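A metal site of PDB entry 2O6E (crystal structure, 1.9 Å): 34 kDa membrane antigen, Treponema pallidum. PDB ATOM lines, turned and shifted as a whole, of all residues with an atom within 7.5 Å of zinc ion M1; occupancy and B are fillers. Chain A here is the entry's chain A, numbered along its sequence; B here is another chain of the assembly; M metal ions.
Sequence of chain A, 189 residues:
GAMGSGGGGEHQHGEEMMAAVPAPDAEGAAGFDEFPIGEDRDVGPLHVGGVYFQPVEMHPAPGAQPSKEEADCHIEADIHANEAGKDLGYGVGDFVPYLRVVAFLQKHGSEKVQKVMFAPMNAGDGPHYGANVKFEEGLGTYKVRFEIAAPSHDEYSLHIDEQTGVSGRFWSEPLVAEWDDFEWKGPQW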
ATOM      1  N   PHE A  32       3.559 -19.112 -18.481  1.00  0.00           N
ATOM      2  CA  PHE A  32       4.603 -19.926 -19.168  1.00  0.00           C
ATOM      3  C   PHE A  32       5.972 -19.281 -18.939  1.00  0.00           C
ATOM      4  O   PHE A  32       6.065 -18.086 -18.568  1.00  0.00           O
ATOM      5  CB  PHE A  32       4.297 -20.077 -20.675  1.00  0.00           C
ATOM      6  CG  PHE A  32       3.783 -18.800 -21.351  1.00  0.00           C
ATOM      7  CD1 PHE A  32       2.446 -18.419 -21.218  1.00  0.00           C
ATOM      8  CD2 PHE A  32       4.627 -18.007 -22.124  1.00  0.00           C
ATOM      9  CE1 PHE A  32       1.946 -17.232 -21.829  1.00  0.00           C
ATOM     10  CE2 PHE A  32       4.146 -16.840 -22.744  1.00  0.00           C
ATOM     11  CZ  PHE A  32       2.800 -16.460 -22.597  1.00  0.00           C
ATOM     12  N   PHE A  53      10.901 -18.538 -26.315  1.00  0.00           N
ATOM     13  CA  PHE A  53      10.518 -19.707 -25.536  1.00  0.00           C
ATOM     14  C   PHE A  53      10.167 -20.805 -26.541  1.00  0.00           C
ATOM     15  O   PHE A  53      10.425 -20.608 -27.725  1.00  0.00           O
ATOM     16  CB  PHE A  53       9.422 -19.413 -24.497  1.00  0.00           C
ATOM     17  CG  PHE A  53       8.265 -18.592 -25.024  1.00  0.00           C
ATOM     18  CD1 PHE A  53       7.180 -19.234 -25.628  1.00  0.00           C
ATOM     19  CD2 PHE A  53       8.247 -17.220 -24.886  1.00  0.00           C
ATOM     20  CE1 PHE A  53       6.095 -18.508 -26.115  1.00  0.00           C
ATOM     21  CE2 PHE A  53       7.154 -16.468 -25.343  1.00  0.00           C
ATOM     22  CZ  PHE A  53       6.069 -17.117 -25.939  1.00  0.00           C
ATOM     23  N   VAL A  56       5.300 -22.387 -30.585  1.00  0.00           N
ATOM     24  CA  VAL A  56       3.873 -22.410 -30.240  1.00  0.00           C
ATOM     25  C   VAL A  56       2.991 -22.751 -31.435  1.00  0.00           C
ATOM     26  O   VAL A  56       3.462 -22.812 -32.574  1.00  0.00           O
ATOM     27  CB  VAL A  56       3.448 -21.056 -29.588  1.00  0.00           C
ATOM     28  CG1 VAL A  56       4.387 -20.697 -28.450  1.00  0.00           C
ATOM     29  CG2 VAL A  56       3.450 -19.942 -30.594  1.00  0.00           C
ATOM     30  N   MET A  58      -0.158 -21.595 -33.549  1.00  0.00           N
ATOM     31  CA  MET A  58      -0.962 -20.405 -33.763  1.00  0.00           C
ATOM     32  C   MET A  58      -2.123 -20.642 -34.706  1.00  0.00           C
ATOM     33  O   MET A  58      -2.011 -21.455 -35.621  1.00  0.00           O
ATOM     34  CB  MET A  58      -0.087 -19.259 -34.288  1.00  0.00           C
ATOM     35  CG  MET A  58       0.937 -18.701 -33.262  1.00  0.00           C
ATOM     36  SD  MET A  58       2.289 -17.896 -34.107  1.00  0.00           S
ATOM     37  CE  MET A  58       3.130 -19.269 -34.892  1.00  0.00           C
ATOM     38  N   HIS A  74       9.933 -19.782 -30.444  1.00  0.00           N
ATOM     39  CA  HIS A  74       8.986 -18.707 -30.738  1.00  0.00           C
ATOM     40  C   HIS A  74       9.649 -17.455 -30.147  1.00  0.00           C
ATOM     41  O   HIS A  74      10.130 -17.479 -29.000  1.00  0.00           O
ATOM     42  CB  HIS A  74       7.656 -18.929 -30.034  1.00  0.00           C
ATOM     43  CG  HIS A  74       6.636 -17.900 -30.391  1.00  0.00           C
ATOM     44  ND1 HIS A  74       6.071 -17.813 -31.644  1.00  0.00           N
ATOM     45  CD2 HIS A  74       6.066 -16.914 -29.650  1.00  0.00           C
ATOM     46  CE1 HIS A  74       5.157 -16.863 -31.656  1.00  0.00           C
ATOM     47  NE2 HIS A  74       5.148 -16.288 -30.455  1.00  0.00           N
ATOM     48  N   ILE A  75       9.760 -16.404 -30.957  1.00  0.00           N
ATOM     49  CA  ILE A  75      10.356 -15.149 -30.527  1.00  0.00           C
ATOM     50  C   ILE A  75       9.262 -14.087 -30.524  1.00  0.00           C
ATOM     51  O   ILE A  75       8.412 -14.043 -31.420  1.00  0.00           O
ATOM     52  CB  ILE A  75      11.527 -14.689 -31.407  1.00  0.00           C
ATOM     53  CG1 ILE A  75      12.717 -15.654 -31.273  1.00  0.00           C
ATOM     54  CG2 ILE A  75      11.941 -13.205 -31.011  1.00  0.00           C
ATOM     55  CD1 ILE A  75      13.920 -15.273 -32.125  1.00  0.00           C
ATOM     56  N   GLU A  76       9.303 -13.208 -29.526  1.00  0.00           N
ATOM     57  CA  GLU A  76       8.324 -12.124 -29.427  1.00  0.00           C
ATOM     58  C   GLU A  76       8.952 -10.752 -29.154  1.00  0.00           C
ATOM     59  O   GLU A  76       9.927 -10.639 -28.388  1.00  0.00           O
ATOM     60  CB  GLU A  76       7.323 -12.408 -28.309  1.00  0.00           C
ATOM     61  CG  GLU A  76       6.453 -13.609 -28.589  1.00  0.00           C
ATOM     62  CD  GLU A  76       5.501 -13.991 -27.494  1.00  0.00           C
ATOM     63  OE1 GLU A  76       5.581 -13.477 -26.336  1.00  0.00           O
ATOM     64  OE2 GLU A  76       4.671 -14.873 -27.776  1.00  0.00           O
ATOM     65  N   ALA A  77       8.325  -9.718 -29.705  1.00  0.00           N
ATOM     66  CA  ALA A  77       8.722  -8.373 -29.466  1.00  0.00           C
ATOM     67  C   ALA A  77       7.553  -7.785 -28.696  1.00  0.00           C
ATOM     68  O   ALA A  77       6.420  -7.767 -29.184  1.00  0.00           O
ATOM     69  CB  ALA A  77       8.921  -7.578 -30.800  1.00  0.00           C
ATOM     70  N   ASP A  78       7.815  -7.324 -27.486  1.00  0.00           N
ATOM     71  CA  ASP A  78       6.779  -6.713 -26.635  1.00  0.00           C
ATOM     72  C   ASP A  78       7.000  -5.202 -26.761  1.00  0.00           C
ATOM     73  O   ASP A  78       7.953  -4.635 -26.220  1.00  0.00           O
ATOM     74  CB  ASP A  78       6.864  -7.258 -25.199  1.00  0.00           C
ATOM     75  CG  ASP A  78       6.810  -8.791 -25.167  1.00  0.00           C
ATOM     76  OD1 ASP A  78       5.809  -9.384 -25.644  1.00  0.00           O
ATOM     77  OD2 ASP A  78       7.793  -9.416 -24.698  1.00  0.00           O
ATOM     78  N   ALA A 119       4.342 -11.335 -36.847  1.00  0.00           N
ATOM     79  CA  ALA A 119       2.920 -11.108 -37.081  1.00  0.00           C
ATOM     80  C   ALA A 119       2.336 -10.626 -35.762  1.00  0.00           C
ATOM     81  O   ALA A 119       2.833 -11.018 -34.731  1.00  0.00           O
ATOM     82  CB  ALA A 119       2.277 -12.409 -37.442  1.00  0.00           C
ATOM     83  N   PRO A 120       1.262  -9.809 -35.783  1.00  0.00           N
ATOM     84  CA  PRO A 120       0.647  -9.446 -34.491  1.00  0.00           C
ATOM     85  C   PRO A 120      -0.240 -10.618 -34.010  1.00  0.00           C
ATOM     86  O   PRO A 120      -0.844 -11.338 -34.817  1.00  0.00           O
ATOM     87  CB  PRO A 120      -0.223  -8.234 -34.829  1.00  0.00           C
ATOM     88  CG  PRO A 120      -0.557  -8.416 -36.294  1.00  0.00           C
ATOM     89  CD  PRO A 120       0.578  -9.175 -36.939  1.00  0.00           C
ATOM     90  N   MET A 121      -0.262 -10.829 -32.703  1.00  0.00           N
ATOM     91  CA  MET A 121      -1.016 -11.962 -32.168  1.00  0.00           C
ATOM     92  C   MET A 121      -1.191 -11.859 -30.679  1.00  0.00           C
ATOM     93  O   MET A 121      -0.484 -11.059 -30.013  1.00  0.00           O
ATOM     94  CB  MET A 121      -0.246 -13.280 -32.493  1.00  0.00           C
ATOM     95  CG  MET A 121       1.110 -13.380 -31.715  1.00  0.00           C
ATOM     96  SD  MET A 121       2.096 -14.846 -32.157  1.00  0.00           S
ATOM     97  CE  MET A 121       2.511 -14.413 -33.836  1.00  0.00           C
ATOM     98  N   ASN A 122      -2.117 -12.645 -30.149  1.00  0.00           N
ATOM     99  CA  ASN A 122      -2.313 -12.709 -28.712  1.00  0.00           C
ATOM    100  C   ASN A 122      -1.805 -14.047 -28.168  1.00  0.00           C
ATOM    101  O   ASN A 122      -2.010 -15.105 -28.801  1.00  0.00           O
ATOM    102  CB  ASN A 122      -3.797 -12.657 -28.310  1.00  0.00           C
ATOM    103  CG  ASN A 122      -4.383 -11.266 -28.337  1.00  0.00           C
ATOM    104  OD1 ASN A 122      -3.718 -10.276 -28.636  1.00  0.00           O
ATOM    105  ND2 ASN A 122      -5.672 -11.186 -28.048  1.00  0.00           N
ATOM    106  N   ALA A 123      -1.213 -13.989 -26.978  1.00  0.00           N
ATOM    107  CA  ALA A 123      -0.794 -15.153 -26.184  1.00  0.00           C
ATOM    108  C   ALA A 123      -1.599 -14.917 -24.892  1.00  0.00           C
ATOM    109  O   ALA A 123      -2.419 -13.993 -24.818  1.00  0.00           O
ATOM    110  CB  ALA A 123       0.709 -15.156 -25.910  1.00  0.00           C
ATOM    111  N   ASP A 125      -0.668 -13.751 -22.305  1.00  0.00           N
ATOM    112  CA  ASP A 125      -0.293 -12.502 -21.674  1.00  0.00           C
ATOM    113  C   ASP A 125      -0.565 -11.263 -22.540  1.00  0.00           C
ATOM    114  O   ASP A 125      -0.045 -10.198 -22.246  1.00  0.00           O
ATOM    115  CB  ASP A 125       1.123 -12.545 -21.108  1.00  0.00           C
ATOM    116  CG  ASP A 125       2.187 -12.654 -22.176  1.00  0.00           C
ATOM    117  OD1 ASP A 125       1.870 -13.157 -23.280  1.00  0.00           O
ATOM    118  OD2 ASP A 125       3.340 -12.240 -21.895  1.00  0.00           O
ATOM    119  N   GLY A 126      -1.410 -11.410 -23.562  1.00  0.00           N
ATOM    120  CA  GLY A 126      -1.830 -10.287 -24.386  1.00  0.00           C
ATOM    121  C   GLY A 126      -1.180 -10.079 -25.742  1.00  0.00           C
ATOM    122  O   GLY A 126      -0.376 -10.894 -26.191  1.00  0.00           O
ATOM    123  N   HIS A 128       1.112  -8.879 -28.865  1.00  0.00           N
ATOM    124  CA  HIS A 128       2.572  -8.651 -29.113  1.00  0.00           C
ATOM    125  C   HIS A 128       2.849  -8.996 -30.580  1.00  0.00           C
ATOM    126  O   HIS A 128       1.939  -9.391 -31.275  1.00  0.00           O
ATOM    127  CB  HIS A 128       3.424  -9.579 -28.239  1.00  0.00           C
ATOM    128  CG  HIS A 128       3.137 -11.030 -28.483  1.00  0.00           C
ATOM    129  ND1 HIS A 128       2.064 -11.691 -27.896  1.00  0.00           N
ATOM    130  CD2 HIS A 128       3.745 -11.942 -29.277  1.00  0.00           C
ATOM    131  CE1 HIS A 128       2.049 -12.940 -28.302  1.00  0.00           C
ATOM    132  NE2 HIS A 128       3.054 -13.112 -29.152  1.00  0.00           N
ATOM    133  N   TYR A 129       4.089  -8.859 -31.059  1.00  0.00           N
ATOM    134  CA  TYR A 129       4.410  -9.217 -32.423  1.00  0.00           C
ATOM    135  C   TYR A 129       5.332 -10.418 -32.257  1.00  0.00           C
ATOM    136  O   TYR A 129       6.135 -10.451 -31.301  1.00  0.00           O
ATOM    137  CB  TYR A 129       5.188  -8.082 -33.107  1.00  0.00           C
ATOM    138  CG  TYR A 129       4.348  -6.820 -33.237  1.00  0.00           C
ATOM    139  CD1 TYR A 129       4.350  -5.858 -32.218  1.00  0.00           C
ATOM    140  CD2 TYR A 129       3.537  -6.613 -34.359  1.00  0.00           C
ATOM    141  CE1 TYR A 129       3.570  -4.695 -32.343  1.00  0.00           C
ATOM    142  CE2 TYR A 129       2.757  -5.457 -34.491  1.00  0.00           C
ATOM    143  CZ  TYR A 129       2.779  -4.531 -33.468  1.00  0.00           C
ATOM    144  OH  TYR A 129       2.011  -3.390 -33.573  1.00  0.00           O
ATOM    145  N   GLY A 130       5.237 -11.411 -33.125  1.00  0.00           N
ATOM    146  CA  GLY A 130       6.170 -12.551 -32.920  1.00  0.00           C
ATOM    147  C   GLY A 130       6.183 -13.556 -34.049  1.00  0.00           C
ATOM    148  O   GLY A 130       5.440 -13.409 -35.014  1.00  0.00           O
ATOM    149  N   ALA A 131       7.042 -14.562 -33.932  1.00  0.00           N
ATOM    150  CA  ALA A 131       7.111 -15.609 -34.945  1.00  0.00           C
ATOM    151  C   ALA A 131       7.749 -16.856 -34.394  1.00  0.00           C
ATOM    152  O   ALA A 131       8.598 -16.763 -33.525  1.00  0.00           O
ATOM    153  CB  ALA A 131       7.987 -15.169 -36.169  1.00  0.00           C
ATOM    154  N   ASN A 132       7.357 -18.004 -34.954  1.00  0.00           N
ATOM    155  CA  ASN A 132       8.043 -19.261 -34.689  1.00  0.00           C
ATOM    156  C   ASN A 132       9.222 -19.057 -35.650  1.00  0.00           C
ATOM    157  O   ASN A 132       9.031 -18.561 -36.759  1.00  0.00           O
ATOM    158  CB  ASN A 132       7.247 -20.473 -35.122  1.00  0.00           C
ATOM    159  CG  ASN A 132       6.305 -20.961 -34.041  1.00  0.00           C
ATOM    160  OD1 ASN A 132       6.293 -20.445 -32.908  1.00  0.00           O
ATOM    161  ND2 ASN A 132       5.523 -21.960 -34.369  1.00  0.00           N
ATOM    162  N   LEU B 158      -3.735 -16.158 -32.815  1.00  0.00           N
ATOM    163  CA  LEU B 158      -3.782 -16.504 -31.402  1.00  0.00           C
ATOM    164  C   LEU B 158      -2.908 -17.702 -31.170  1.00  0.00           C
ATOM    165  O   LEU B 158      -2.890 -18.656 -31.984  1.00  0.00           O
ATOM    166  CB  LEU B 158      -5.222 -16.866 -30.943  1.00  0.00           C
ATOM    167  CG  LEU B 158      -6.347 -15.851 -31.190  1.00  0.00           C
ATOM    168  CD1 LEU B 158      -7.732 -16.461 -30.863  1.00  0.00           C
ATOM    169  CD2 LEU B 158      -6.115 -14.536 -30.385  1.00  0.00           C
ATOM    170  N   HIS B 159      -2.198 -17.695 -30.059  1.00  0.00           N
ATOM    171  CA  HIS B 159      -1.416 -18.870 -29.644  1.00  0.00           C
ATOM    172  C   HIS B 159      -2.573 -19.779 -29.169  1.00  0.00           C
ATOM    173  O   HIS B 159      -3.463 -19.302 -28.433  1.00  0.00           O
ATOM    174  CB  HIS B 159      -0.651 -18.575 -28.389  1.00  0.00           C
ATOM    175  CG  HIS B 159       0.621 -17.820 -28.560  1.00  0.00           C
ATOM    176  ND1 HIS B 159       1.690 -18.010 -27.704  1.00  0.00           N
ATOM    177  CD2 HIS B 159       0.981 -16.830 -29.406  1.00  0.00           C
ATOM    178  CE1 HIS B 159       2.655 -17.153 -28.018  1.00  0.00           C
ATOM    179  NE2 HIS B 159       2.247 -16.429 -29.039  1.00  0.00           N
ATOM    180  N   THR B 164       0.926 -21.972 -23.705  1.00  0.00           N
ATOM    181  CA  THR B 164       1.046 -20.518 -23.844  1.00  0.00           C
ATOM    182  C   THR B 164      -0.209 -19.765 -24.322  1.00  0.00           C
ATOM    183  O   THR B 164      -0.236 -18.576 -24.408  1.00  0.00           O
ATOM    184  CB  THR B 164       2.227 -20.135 -24.737  1.00  0.00           C
ATOM    185  OG1 THR B 164       1.887 -20.317 -26.095  1.00  0.00           O
ATOM    186  CG2 THR B 164       3.485 -20.993 -24.394  1.00  0.00           C
HETATM  187 ZN    ZN M   1       3.652 -15.127 -29.563  1.00  0.00          ZN
HETATM  188 ZN    ZN M   2       5.472 -11.975 -23.469  1.00  0.00          ZN
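NE2 of His 159 of chain B sits close to SD of Met 121 (3.5 Å).
A ring nitrogen (ND1) of His 159 of chain B lies within hydrogen-bond range of the side-chain hydroxyl (OG1) of Thr 164 of chain B, at 2.8 Å.
NE2 of His 74 lies close to SD of Met 121.
N of His 74 lies within hydrogen-bond range of O of Phe 53, 2.9 Å away.
A ring nitrogen (ND1) of His 74 is in hydrogen-bond range of the backbone carbonyl oxygen (O) of Ala 131, 3.3 Å away.
The side-chain amide oxygen (OD1) of Asn 132 lies within hydrogen-bond range of a ring nitrogen (ND1) of His 74 (2.9 Å).
N of His 128 is in hydrogen-bond range of O of Met 121, at 2.9 Å.
ND1 of His 128 sits at hydrogen-bond distance from O of Gly 126 (3.1 Å).
Zinc ion M1 is bound by a ring nitrogen (NE2) of His 159 of chain B (2.0 Å), the side-chain carboxylate of Glu 76 (2.1 Å), a ring nitrogen (NE2) of His 74 (2.1 Å) and a ring nitrogen (NE2) of His 128 (2.1 Å).
Zinc ion M1 has four donor atoms within binding distance.
Slightly farther from zinc ion M1 lies the side-chain sulfur (SD) of Met 121 (3.0 Å).
Of the 24 residues printed, 5 come within 4 Å of zinc ion M1.
Along chain A the residues within 4 Å of zinc ion M1 span positions 74 to 128.
The nearest printed residue that does not touch zinc ion M1 is Ala 123 (4.7 Å).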
